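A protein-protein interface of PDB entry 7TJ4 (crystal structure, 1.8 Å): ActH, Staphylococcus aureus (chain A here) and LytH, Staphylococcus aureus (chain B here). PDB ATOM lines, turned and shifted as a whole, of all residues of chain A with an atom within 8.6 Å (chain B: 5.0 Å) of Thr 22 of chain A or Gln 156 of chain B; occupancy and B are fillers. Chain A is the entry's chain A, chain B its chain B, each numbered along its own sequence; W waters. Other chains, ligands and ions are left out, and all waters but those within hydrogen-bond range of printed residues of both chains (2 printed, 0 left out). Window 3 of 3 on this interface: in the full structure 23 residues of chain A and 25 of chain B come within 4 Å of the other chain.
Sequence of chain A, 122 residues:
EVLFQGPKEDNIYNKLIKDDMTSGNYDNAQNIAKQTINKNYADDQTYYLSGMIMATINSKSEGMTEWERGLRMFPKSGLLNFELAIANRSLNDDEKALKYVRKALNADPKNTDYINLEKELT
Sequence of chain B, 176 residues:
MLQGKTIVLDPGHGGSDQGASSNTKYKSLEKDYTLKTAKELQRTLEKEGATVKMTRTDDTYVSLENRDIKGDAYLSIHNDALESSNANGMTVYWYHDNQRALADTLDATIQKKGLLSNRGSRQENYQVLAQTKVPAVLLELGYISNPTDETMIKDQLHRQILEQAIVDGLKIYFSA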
ATOM      1  N   LYS A  15     -17.886  24.475  -1.537  1.00  0.00           N
ATOM      2  CA  LYS A  15     -19.052  24.461  -0.669  1.00  0.00           C
ATOM      3  C   LYS A  15     -20.344  24.645  -1.461  1.00  0.00           C
ATOM      4  O   LYS A  15     -21.326  23.923  -1.233  1.00  0.00           O
ATOM      5  CB  LYS A  15     -18.946  25.506   0.415  1.00  0.00           C
ATOM      6  CG  LYS A  15     -20.260  25.582   1.092  1.00  0.00           C
ATOM      7  CD  LYS A  15     -20.223  26.354   2.359  1.00  0.00           C
ATOM      8  CE  LYS A  15     -21.623  26.464   2.940  1.00  0.00           C
ATOM      9  NZ  LYS A  15     -21.601  27.580   3.888  1.00  0.00           N
ATOM     10  N   LEU A  16     -20.353  25.553  -2.443  1.00  0.00           N
ATOM     11  CA  LEU A  16     -21.551  25.752  -3.256  1.00  0.00           C
ATOM     12  C   LEU A  16     -21.879  24.516  -4.087  1.00  0.00           C
ATOM     13  O   LEU A  16     -23.047  24.121  -4.211  1.00  0.00           O
ATOM     14  CB  LEU A  16     -21.385  26.968  -4.170  1.00  0.00           C
ATOM     15  CG  LEU A  16     -21.398  28.289  -3.423  1.00  0.00           C
ATOM     16  CD1 LEU A  16     -20.805  29.430  -4.307  1.00  0.00           C
ATOM     17  CD2 LEU A  16     -22.851  28.575  -3.023  1.00  0.00           C
ATOM     18  N   ILE A  17     -20.868  23.885  -4.652  1.00  0.00           N
ATOM     19  CA  ILE A  17     -21.103  22.684  -5.423  1.00  0.00           C
ATOM     20  C   ILE A  17     -21.705  21.604  -4.534  1.00  0.00           C
ATOM     21  O   ILE A  17     -22.667  20.931  -4.909  1.00  0.00           O
ATOM     22  CB  ILE A  17     -19.797  22.201  -6.044  1.00  0.00           C
ATOM     23  CG1 ILE A  17     -19.326  23.167  -7.130  1.00  0.00           C
ATOM     24  CG2 ILE A  17     -19.954  20.818  -6.596  1.00  0.00           C
ATOM     25  CD1 ILE A  17     -17.874  22.997  -7.409  1.00  0.00           C
ATOM     26  N   LYS A  18     -21.111  21.400  -3.358  1.00  0.00           N
ATOM     27  CA  LYS A  18     -21.572  20.338  -2.462  1.00  0.00           C
ATOM     28  C   LYS A  18     -22.988  20.592  -2.007  1.00  0.00           C
ATOM     29  O   LYS A  18     -23.795  19.667  -1.946  1.00  0.00           O
ATOM     30  CB  LYS A  18     -20.676  20.233  -1.244  1.00  0.00           C
ATOM     31  CG  LYS A  18     -19.395  19.487  -1.464  1.00  0.00           C
ATOM     32  CD  LYS A  18     -18.537  19.592  -0.212  1.00  0.00           C
ATOM     33  CE  LYS A  18     -18.142  18.233   0.283  1.00  0.00           C
ATOM     34  NZ  LYS A  18     -17.198  18.369   1.452  1.00  0.00           N
ATOM     35  N   ASP A  19     -23.301  21.842  -1.684  1.00  0.00           N
ATOM     36  CA  ASP A  19     -24.627  22.174  -1.188  1.00  0.00           C
ATOM     37  C   ASP A  19     -25.699  21.923  -2.248  1.00  0.00           C
ATOM     38  O   ASP A  19     -26.794  21.464  -1.913  1.00  0.00           O
ATOM     39  CB  ASP A  19     -24.643  23.629  -0.690  1.00  0.00           C
ATOM     40  CG  ASP A  19     -24.064  23.751   0.733  1.00  0.00           C
ATOM     41  OD1 ASP A  19     -23.562  22.702   1.267  1.00  0.00           O
ATOM     42  OD2 ASP A  19     -24.152  24.857   1.330  1.00  0.00           O
ATOM     43  N   ASP A  20     -25.398  22.176  -3.533  1.00  0.00           N
ATOM     44  CA  ASP A  20     -26.354  21.815  -4.586  1.00  0.00           C
ATOM     45  C   ASP A  20     -26.469  20.299  -4.745  1.00  0.00           C
ATOM     46  O   ASP A  20     -27.560  19.776  -5.022  1.00  0.00           O
ATOM     47  CB  ASP A  20     -25.948  22.420  -5.913  1.00  0.00           C
ATOM     48  CG  ASP A  20     -26.312  23.913  -6.018  1.00  0.00           C
ATOM     49  OD1 ASP A  20     -27.274  24.367  -5.338  1.00  0.00           O
ATOM     50  OD2 ASP A  20     -25.622  24.621  -6.786  1.00  0.00           O
ATOM     51  N   MET A  21     -25.357  19.592  -4.591  1.00  0.00           N
ATOM     52  CA  MET A  21     -25.376  18.136  -4.727  1.00  0.00           C
ATOM     53  C   MET A  21     -26.213  17.492  -3.635  1.00  0.00           C
ATOM     54  O   MET A  21     -27.014  16.597  -3.937  1.00  0.00           O
ATOM     55  CB  MET A  21     -23.971  17.551  -4.713  1.00  0.00           C
ATOM     56  CG  MET A  21     -23.111  17.922  -5.929  1.00  0.00           C
ATOM     57  SD  MET A  21     -21.450  17.260  -5.690  1.00  0.00           S
ATOM     58  CE  MET A  21     -21.600  15.445  -5.894  1.00  0.00           C
ATOM     59  N   THR A  22     -26.066  17.941  -2.372  1.00  0.00           N
ATOM     60  CA  THR A  22     -26.785  17.314  -1.269  1.00  0.00           C
ATOM     61  C   THR A  22     -28.231  17.764  -1.204  1.00  0.00           C
ATOM     62  O   THR A  22     -29.026  17.118  -0.542  1.00  0.00           O
ATOM     63  CB  THR A  22     -26.094  17.555   0.093  1.00  0.00           C
ATOM     64  OG1 THR A  22     -25.870  18.951   0.310  1.00  0.00           O
ATOM     65  CG2 THR A  22     -24.720  16.808   0.144  1.00  0.00           C
ATOM     66  N   SER A  23     -28.603  18.827  -1.901  1.00  0.00           N
ATOM     67  CA  SER A  23     -30.007  19.183  -2.012  1.00  0.00           C
ATOM     68  C   SER A  23     -30.635  18.616  -3.283  1.00  0.00           C
ATOM     69  O   SER A  23     -31.805  18.920  -3.580  1.00  0.00           O
ATOM     70  CB  SER A  23     -30.169  20.705  -1.947  1.00  0.00           C
ATOM     71  OG  SER A  23     -29.428  21.320  -2.999  1.00  0.00           O
ATOM     72  N   GLY A  24     -29.878  17.801  -4.027  1.00  0.00           N
ATOM     73  CA  GLY A  24     -30.343  17.155  -5.243  1.00  0.00           C
ATOM     74  C   GLY A  24     -30.473  18.058  -6.448  1.00  0.00           C
ATOM     75  O   GLY A  24     -31.240  17.750  -7.364  1.00  0.00           O
ATOM     76  N   ASN A  25     -29.768  19.180  -6.466  1.00  0.00           N
ATOM     77  CA  ASN A  25     -29.788  20.075  -7.616  1.00  0.00           C
ATOM     78  C   ASN A  25     -28.489  19.903  -8.400  1.00  0.00           C
ATOM     79  O   ASN A  25     -27.644  20.798  -8.493  1.00  0.00           O
ATOM     80  CB  ASN A  25     -29.998  21.513  -7.162  1.00  0.00           C
ATOM     81  CG  ASN A  25     -31.328  21.699  -6.500  1.00  0.00           C
ATOM     82  OD1 ASN A  25     -32.343  21.853  -7.176  1.00  0.00           O
ATOM     83  ND2 ASN A  25     -31.350  21.645  -5.178  1.00  0.00           N
ATOM     84  N   TYR A  26     -28.364  18.702  -8.965  1.00  0.00           N
ATOM     85  CA  TYR A  26     -27.167  18.319  -9.688  1.00  0.00           C
ATOM     86  C   TYR A  26     -26.985  19.153 -10.958  1.00  0.00           C
ATOM     87  O   TYR A  26     -25.865  19.308 -11.437  1.00  0.00           O
ATOM     88  CB  TYR A  26     -27.220  16.813  -9.976  1.00  0.00           C
ATOM     89  CG  TYR A  26     -26.776  15.996  -8.781  1.00  0.00           C
ATOM     90  CD1 TYR A  26     -27.686  15.554  -7.799  1.00  0.00           C
ATOM     91  CD2 TYR A  26     -25.460  15.653  -8.639  1.00  0.00           C
ATOM     92  CE1 TYR A  26     -27.252  14.793  -6.673  1.00  0.00           C
ATOM     93  CE2 TYR A  26     -24.996  14.917  -7.529  1.00  0.00           C
ATOM     94  CZ  TYR A  26     -25.878  14.480  -6.531  1.00  0.00           C
ATOM     95  OH  TYR A  26     -25.335  13.726  -5.420  1.00  0.00           O
ATOM     96  N   ALA A  29     -25.236  22.187  -9.618  1.00  0.00           N
ATOM     97  CA  ALA A  29     -23.913  21.768  -9.159  1.00  0.00           C
ATOM     98  C   ALA A  29     -22.945  21.667 -10.327  1.00  0.00           C
ATOM     99  O   ALA A  29     -21.802  22.122 -10.232  1.00  0.00           O
ATOM    100  CB  ALA A  29     -23.978  20.423  -8.441  1.00  0.00           C
ATOM    101  N   TYR A  48     -12.817  16.255  -8.119  1.00  0.00           N
ATOM    102  CA  TYR A  48     -13.510  15.167  -7.431  1.00  0.00           C
ATOM    103  C   TYR A  48     -15.025  15.344  -7.489  1.00  0.00           C
ATOM    104  O   TYR A  48     -15.754  14.460  -7.979  1.00  0.00           O
ATOM    105  CB  TYR A  48     -13.023  15.086  -5.987  1.00  0.00           C
ATOM    106  CG  TYR A  48     -13.858  14.171  -5.121  1.00  0.00           C
ATOM    107  CD1 TYR A  48     -13.683  12.775  -5.166  1.00  0.00           C
ATOM    108  CD2 TYR A  48     -14.816  14.679  -4.264  1.00  0.00           C
ATOM    109  CE1 TYR A  48     -14.465  11.896  -4.385  1.00  0.00           C
ATOM    110  CE2 TYR A  48     -15.612  13.773  -3.441  1.00  0.00           C
ATOM    111  CZ  TYR A  48     -15.403  12.387  -3.530  1.00  0.00           C
ATOM    112  OH  TYR A  48     -16.154  11.500  -2.780  1.00  0.00           O
ATOM    113  N   LEU A  49     -15.509  16.489  -7.010  1.00  0.00           N
ATOM    114  CA  LEU A  49     -16.939  16.716  -6.987  1.00  0.00           C
ATOM    115  C   LEU A  49     -17.513  16.703  -8.386  1.00  0.00           C
ATOM    116  O   LEU A  49     -18.637  16.212  -8.603  1.00  0.00           O
ATOM    117  CB  LEU A  49     -17.267  18.031  -6.272  1.00  0.00           C
ATOM    118  CG  LEU A  49     -16.943  18.131  -4.782  1.00  0.00           C
ATOM    119  CD1 LEU A  49     -17.152  19.577  -4.338  1.00  0.00           C
ATOM    120  CD2 LEU A  49     -17.837  17.133  -3.952  1.00  0.00           C
ATOM    121  N   MET A  52     -17.938  13.212  -9.440  1.00  0.00           N
ATOM    122  CA  MET A  52     -19.027  12.588  -8.658  1.00  0.00           C
ATOM    123  C   MET A  52     -20.380  12.965  -9.231  1.00  0.00           C
ATOM    124  O   MET A  52     -21.295  12.146  -9.304  1.00  0.00           O
ATOM    125  CB  MET A  52     -18.990  13.024  -7.183  1.00  0.00           C
ATOM    126  CG  MET A  52     -17.856  12.478  -6.391  1.00  0.00           C
ATOM    127  SD  MET A  52     -17.953  10.638  -6.164  1.00  0.00           S
ATOM    128  CE  MET A  52     -19.164  10.538  -4.863  1.00  0.00           C
ATOM    129  N   ILE A  53     -20.524  14.224  -9.619  1.00  0.00           N
ATOM    130  CA  ILE A  53     -21.729  14.677 -10.292  1.00  0.00           C
ATOM    131  C   ILE A  53     -21.963  13.885 -11.564  1.00  0.00           C
ATOM    132  O   ILE A  53     -23.100  13.532 -11.910  1.00  0.00           O
ATOM    133  CB  ILE A  53     -21.595  16.180 -10.614  1.00  0.00           C
ATOM    134  CG1 ILE A  53     -21.698  16.981  -9.322  1.00  0.00           C
ATOM    135  CG2 ILE A  53     -22.699  16.606 -11.594  1.00  0.00           C
ATOM    136  CD1 ILE A  53     -21.200  18.467  -9.538  1.00  0.00           C
ATOM    137  N   THR A  56     -23.199  10.563 -10.970  1.00  0.00           N
ATOM    138  CA  THR A  56     -24.577  10.562 -10.526  1.00  0.00           C
ATOM    139  C   THR A  56     -25.549  10.754 -11.659  1.00  0.00           C
ATOM    140  O   THR A  56     -26.597  10.109 -11.677  1.00  0.00           O
ATOM    141  CB  THR A  56     -24.799  11.651  -9.495  1.00  0.00           C
ATOM    142  OG1 THR A  56     -23.803  11.524  -8.478  1.00  0.00           O
ATOM    143  CG2 THR A  56     -26.211  11.546  -8.928  1.00  0.00           C
ATOM    144  N   GLU B  40     -32.999   9.090   2.037  1.00  0.00           N
ATOM    145  CA  GLU B  40     -32.519   9.832   0.862  1.00  0.00           C
ATOM    146  C   GLU B  40     -33.251   9.393  -0.408  1.00  0.00           C
ATOM    147  O   GLU B  40     -33.722  10.221  -1.204  1.00  0.00           O
ATOM    148  CB  GLU B  40     -31.017   9.625   0.738  1.00  0.00           C
ATOM    149  CG  GLU B  40     -30.302  10.411   1.816  1.00  0.00           C
ATOM    150  CD  GLU B  40     -28.857   9.941   2.041  1.00  0.00           C
ATOM    151  OE1 GLU B  40     -28.482   8.884   1.452  1.00  0.00           O
ATOM    152  OE2 GLU B  40     -28.087  10.646   2.786  1.00  0.00           O
ATOM    153  N   LYS B 154     -20.789   5.260   4.354  1.00  0.00           N
ATOM    154  CA  LYS B 154     -20.737   6.399   5.248  1.00  0.00           C
ATOM    155  C   LYS B 154     -20.799   7.740   4.506  1.00  0.00           C
ATOM    156  O   LYS B 154     -21.016   8.752   5.159  1.00  0.00           O
ATOM    157  CB  LYS B 154     -19.421   6.362   6.055  1.00  0.00           C
ATOM    158  CG  LYS B 154     -19.506   5.858   7.473  1.00  0.00           C
ATOM    159  CD  LYS B 154     -18.221   6.318   8.259  1.00  0.00           C
ATOM    160  CE  LYS B 154     -16.942   6.213   7.391  1.00  0.00           C
ATOM    161  NZ  LYS B 154     -16.043   7.467   7.187  1.00  0.00           N
ATOM    162  N   ASP B 155     -20.710   7.767   3.191  1.00  0.00           N
ATOM    163  CA  ASP B 155     -20.589   9.014   2.437  1.00  0.00           C
ATOM    164  C   ASP B 155     -21.856   9.362   1.665  1.00  0.00           C
ATOM    165  O   ASP B 155     -22.184   8.691   0.684  1.00  0.00           O
ATOM    166  CB  ASP B 155     -19.420   8.929   1.461  1.00  0.00           C
ATOM    167  CG  ASP B 155     -19.242  10.236   0.676  1.00  0.00           C
ATOM    168  OD1 ASP B 155     -19.123  11.309   1.325  1.00  0.00           O
ATOM    169  OD2 ASP B 155     -19.200  10.179  -0.550  1.00  0.00           O
ATOM    170  N   GLN B 156     -22.506  10.472   2.035  1.00  0.00           N
ATOM    171  CA  GLN B 156     -23.748  10.854   1.357  1.00  0.00           C
ATOM    172  C   GLN B 156     -23.586  10.989  -0.161  1.00  0.00           C
ATOM    173  O   GLN B 156     -24.470  10.562  -0.925  1.00  0.00           O
ATOM    174  CB  GLN B 156     -24.300  12.143   1.960  1.00  0.00           C
ATOM    175  CG  GLN B 156     -25.640  12.616   1.353  1.00  0.00           C
ATOM    176  CD  GLN B 156     -26.329  13.639   2.253  1.00  0.00           C
ATOM    177  OE1 GLN B 156     -25.760  14.686   2.553  1.00  0.00           O
ATOM    178  NE2 GLN B 156     -27.541  13.283   2.778  1.00  0.00           N
ATOM    179  N   LEU B 157     -22.482  11.555  -0.636  1.00  0.00           N
ATOM    180  CA  LEU B 157     -22.344  11.722  -2.092  1.00  0.00           C
ATOM    181  C   LEU B 157     -22.241  10.372  -2.816  1.00  0.00           C
ATOM    182  O   LEU B 157     -22.831  10.181  -3.891  1.00  0.00           O
ATOM    183  CB  LEU B 157     -21.117  12.602  -2.405  1.00  0.00           C
ATOM    184  CG  LEU B 157     -21.160  14.021  -1.852  1.00  0.00           C
ATOM    185  CD1 LEU B 157     -19.947  14.829  -2.450  1.00  0.00           C
ATOM    186  CD2 LEU B 157     -22.557  14.598  -2.172  1.00  0.00           C
ATOM    187  N   HIS B 158     -21.528   9.406  -2.244  1.00  0.00           N
ATOM    188  CA  HIS B 158     -21.572   8.078  -2.867  1.00  0.00           C
ATOM    189  C   HIS B 158     -22.954   7.450  -2.785  1.00  0.00           C
ATOM    190  O   HIS B 158     -23.427   6.913  -3.778  1.00  0.00           O
ATOM    191  CB  HIS B 158     -20.546   7.149  -2.245  1.00  0.00           C
ATOM    192  CG  HIS B 158     -19.161   7.423  -2.705  1.00  0.00           C
ATOM    193  ND1 HIS B 158     -18.363   8.393  -2.129  1.00  0.00           N
ATOM    194  CD2 HIS B 158     -18.458   6.915  -3.742  1.00  0.00           C
ATOM    195  CE1 HIS B 158     -17.202   8.430  -2.769  1.00  0.00           C
ATOM    196  NE2 HIS B 158     -17.236   7.543  -3.749  1.00  0.00           N
ATOM    197  N   ARG B 159     -23.606   7.511  -1.630  1.00  0.00           N
ATOM    198  CA  ARG B 159     -24.980   6.978  -1.521  1.00  0.00           C
ATOM    199  C   ARG B 159     -25.890   7.574  -2.577  1.00  0.00           C
ATOM    200  O   ARG B 159     -26.732   6.872  -3.162  1.00  0.00           O
ATOM    201  CB  ARG B 159     -25.545   7.276  -0.152  1.00  0.00           C
ATOM    202  CG  ARG B 159     -24.900   6.425   0.916  1.00  0.00           C
ATOM    203  CD  ARG B 159     -25.752   6.338   2.168  1.00  0.00           C
ATOM    204  NE  ARG B 159     -26.120   7.635   2.732  1.00  0.00           N
ATOM    205  CZ  ARG B 159     -25.390   8.315   3.602  1.00  0.00           C
ATOM    206  NH1 ARG B 159     -24.269   7.822   4.114  1.00  0.00           N
ATOM    207  NH2 ARG B 159     -25.769   9.540   3.937  1.00  0.00           N
ATOM    208  N   GLN B 160     -25.688   8.853  -2.907  1.00  0.00           N
ATOM    209  CA  GLN B 160     -26.631   9.510  -3.804  1.00  0.00           C
ATOM    210  C   GLN B 160     -26.418   9.071  -5.237  1.00  0.00           C
ATOM    211  O   GLN B 160     -27.332   9.196  -6.052  1.00  0.00           O
ATOM    212  CB  GLN B 160     -26.534  11.036  -3.654  1.00  0.00           C
ATOM    213  CG  GLN B 160     -27.213  11.450  -2.328  1.00  0.00           C
ATOM    214  CD  GLN B 160     -27.291  12.957  -2.112  1.00  0.00           C
ATOM    215  OE1 GLN B 160     -26.553  13.741  -2.741  1.00  0.00           O
ATOM    216  NE2 GLN B 160     -28.163  13.373  -1.198  1.00  0.00           N
HETATM  217  O   HOH W   1     -17.908  12.580  -1.036  1.00  0.00           O
HETATM  218  O   HOH W   2     -23.404  12.216  -5.711  1.00  0.00           O
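The side-chain hydroxyl of Tyr 26 of chain A sits at hydrogen-bond distance from the side-chain amide oxygen of Gln 160 of chain B, 2.9 Å away. O of Met 21 of chain A lies close to OE1 of Gln 160 of chain B, 3.1 Å away.
The side-chain carboxylate (OE2) of Glu 40 of chain B is in hydrogen-bond range of the side-chain amide nitrogen (NE2) of Gln 156 of chain B, at 2.7 Å. OD2 of Asp 155 of chain B is in hydrogen-bond range of ND1 of His 158 of chain B (2.5 Å). The backbone carbonyl oxygen (O) of Met 52 of chain A is in hydrogen-bond range of the side-chain hydroxyl (OG1) of Thr 56 of chain A. O of Lys 18 of chain A lies within hydrogen-bond range of OG1 of Thr 22 of chain A (3.1 Å). OG1 of Thr 22 of chain A lies within hydrogen-bond range of O of Asp 19 of chain A.
Leu 157 of chain B touches Met 21 of chain A (CD1 to CE, 3.9 Å). Thr 22 of chain A touches Gln 156 of chain B. CG2 of Thr 22 of chain A touches CD2 of Leu 157 of chain B (3.9 Å). Thr 22 of chain A touches Gln 160 of chain B (CA to OE1, 3.9 Å). Tyr 48 of chain A touches Asp 155 of chain B (OH to OD2, 3.9995 Å). Tyr 48 of chain A touches His 158 of chain B. Leu 157 of chain B touches Leu 49 of chain A. Met 52 of chain A touches Leu 157 of chain B. CE1 of His 158 of chain B touches CE of Met 52 of chain A, at 3.6 Å. O of Gln 160 of chain B touches CG2 of Thr 56 of chain A, at 3.9 Å.
Of the printed residues of chain B, Thr 22 of chain A touches Gln 156 (3.4 Å), Leu 157 (3.9 Å) and Gln 160 (3.9 Å). Of the printed residues of chain A, Gln 156 of chain B touches Thr 22. Of the printed residues of chain A, Gln 160 of chain B touches Met 21 (3.1 Å), Thr 22 (3.9 Å), Tyr 26 (2.9 Å) and Thr 56 (3.9 Å). Printed residues of chain B within 4 Å of Tyr 26 of chain A: Gln 160. Of the printed residues of chain B, Met 52 of chain A touches Leu 157 (3.7 Å) and His 158 (3.6 Å). The nearest printed residue of chain A that does not touch Leu 157 of chain B is Tyr 26 of chain A (4.4 Å).
Printed residues of chain B that touch a printed residue of chain A: Asp 155, Gln 156, Leu 157, His 158 and Gln 160. Hydrophobic or aromatic side chains of chain B within 4 Å of the printed part of chain A: Leu 157 and His 158. Along chain B the printed residues that touch a printed residue of chain A span positions 155 to 160. Of the 18 printed residues of chain A, 7 touch a printed residue of chain B. Printed residues of chain A that touch a printed residue of chain B: Met 21, Thr 22, Tyr 26, Tyr 48, Leu 49, Met 52 and Thr 56. Among the printed residues, 12 pairs touch across the chains. Among the printed residues, no Asp or Glu carboxylate lies within 4 Å of a Lys or Arg side-chain nitrogen of the other chain.
Water W2 lies within hydrogen-bond range of OH of Tyr 26 of chain A (2.5 Å), O of Leu 157 of chain B (2.8 Å) and OG1 of Thr 56 of chain A (2.9 Å). Water W1 lies within hydrogen-bond range of OH of Tyr 48 of chain A (2.7 Å) and OD2 of Asp 155 of chain B (2.8 Å).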
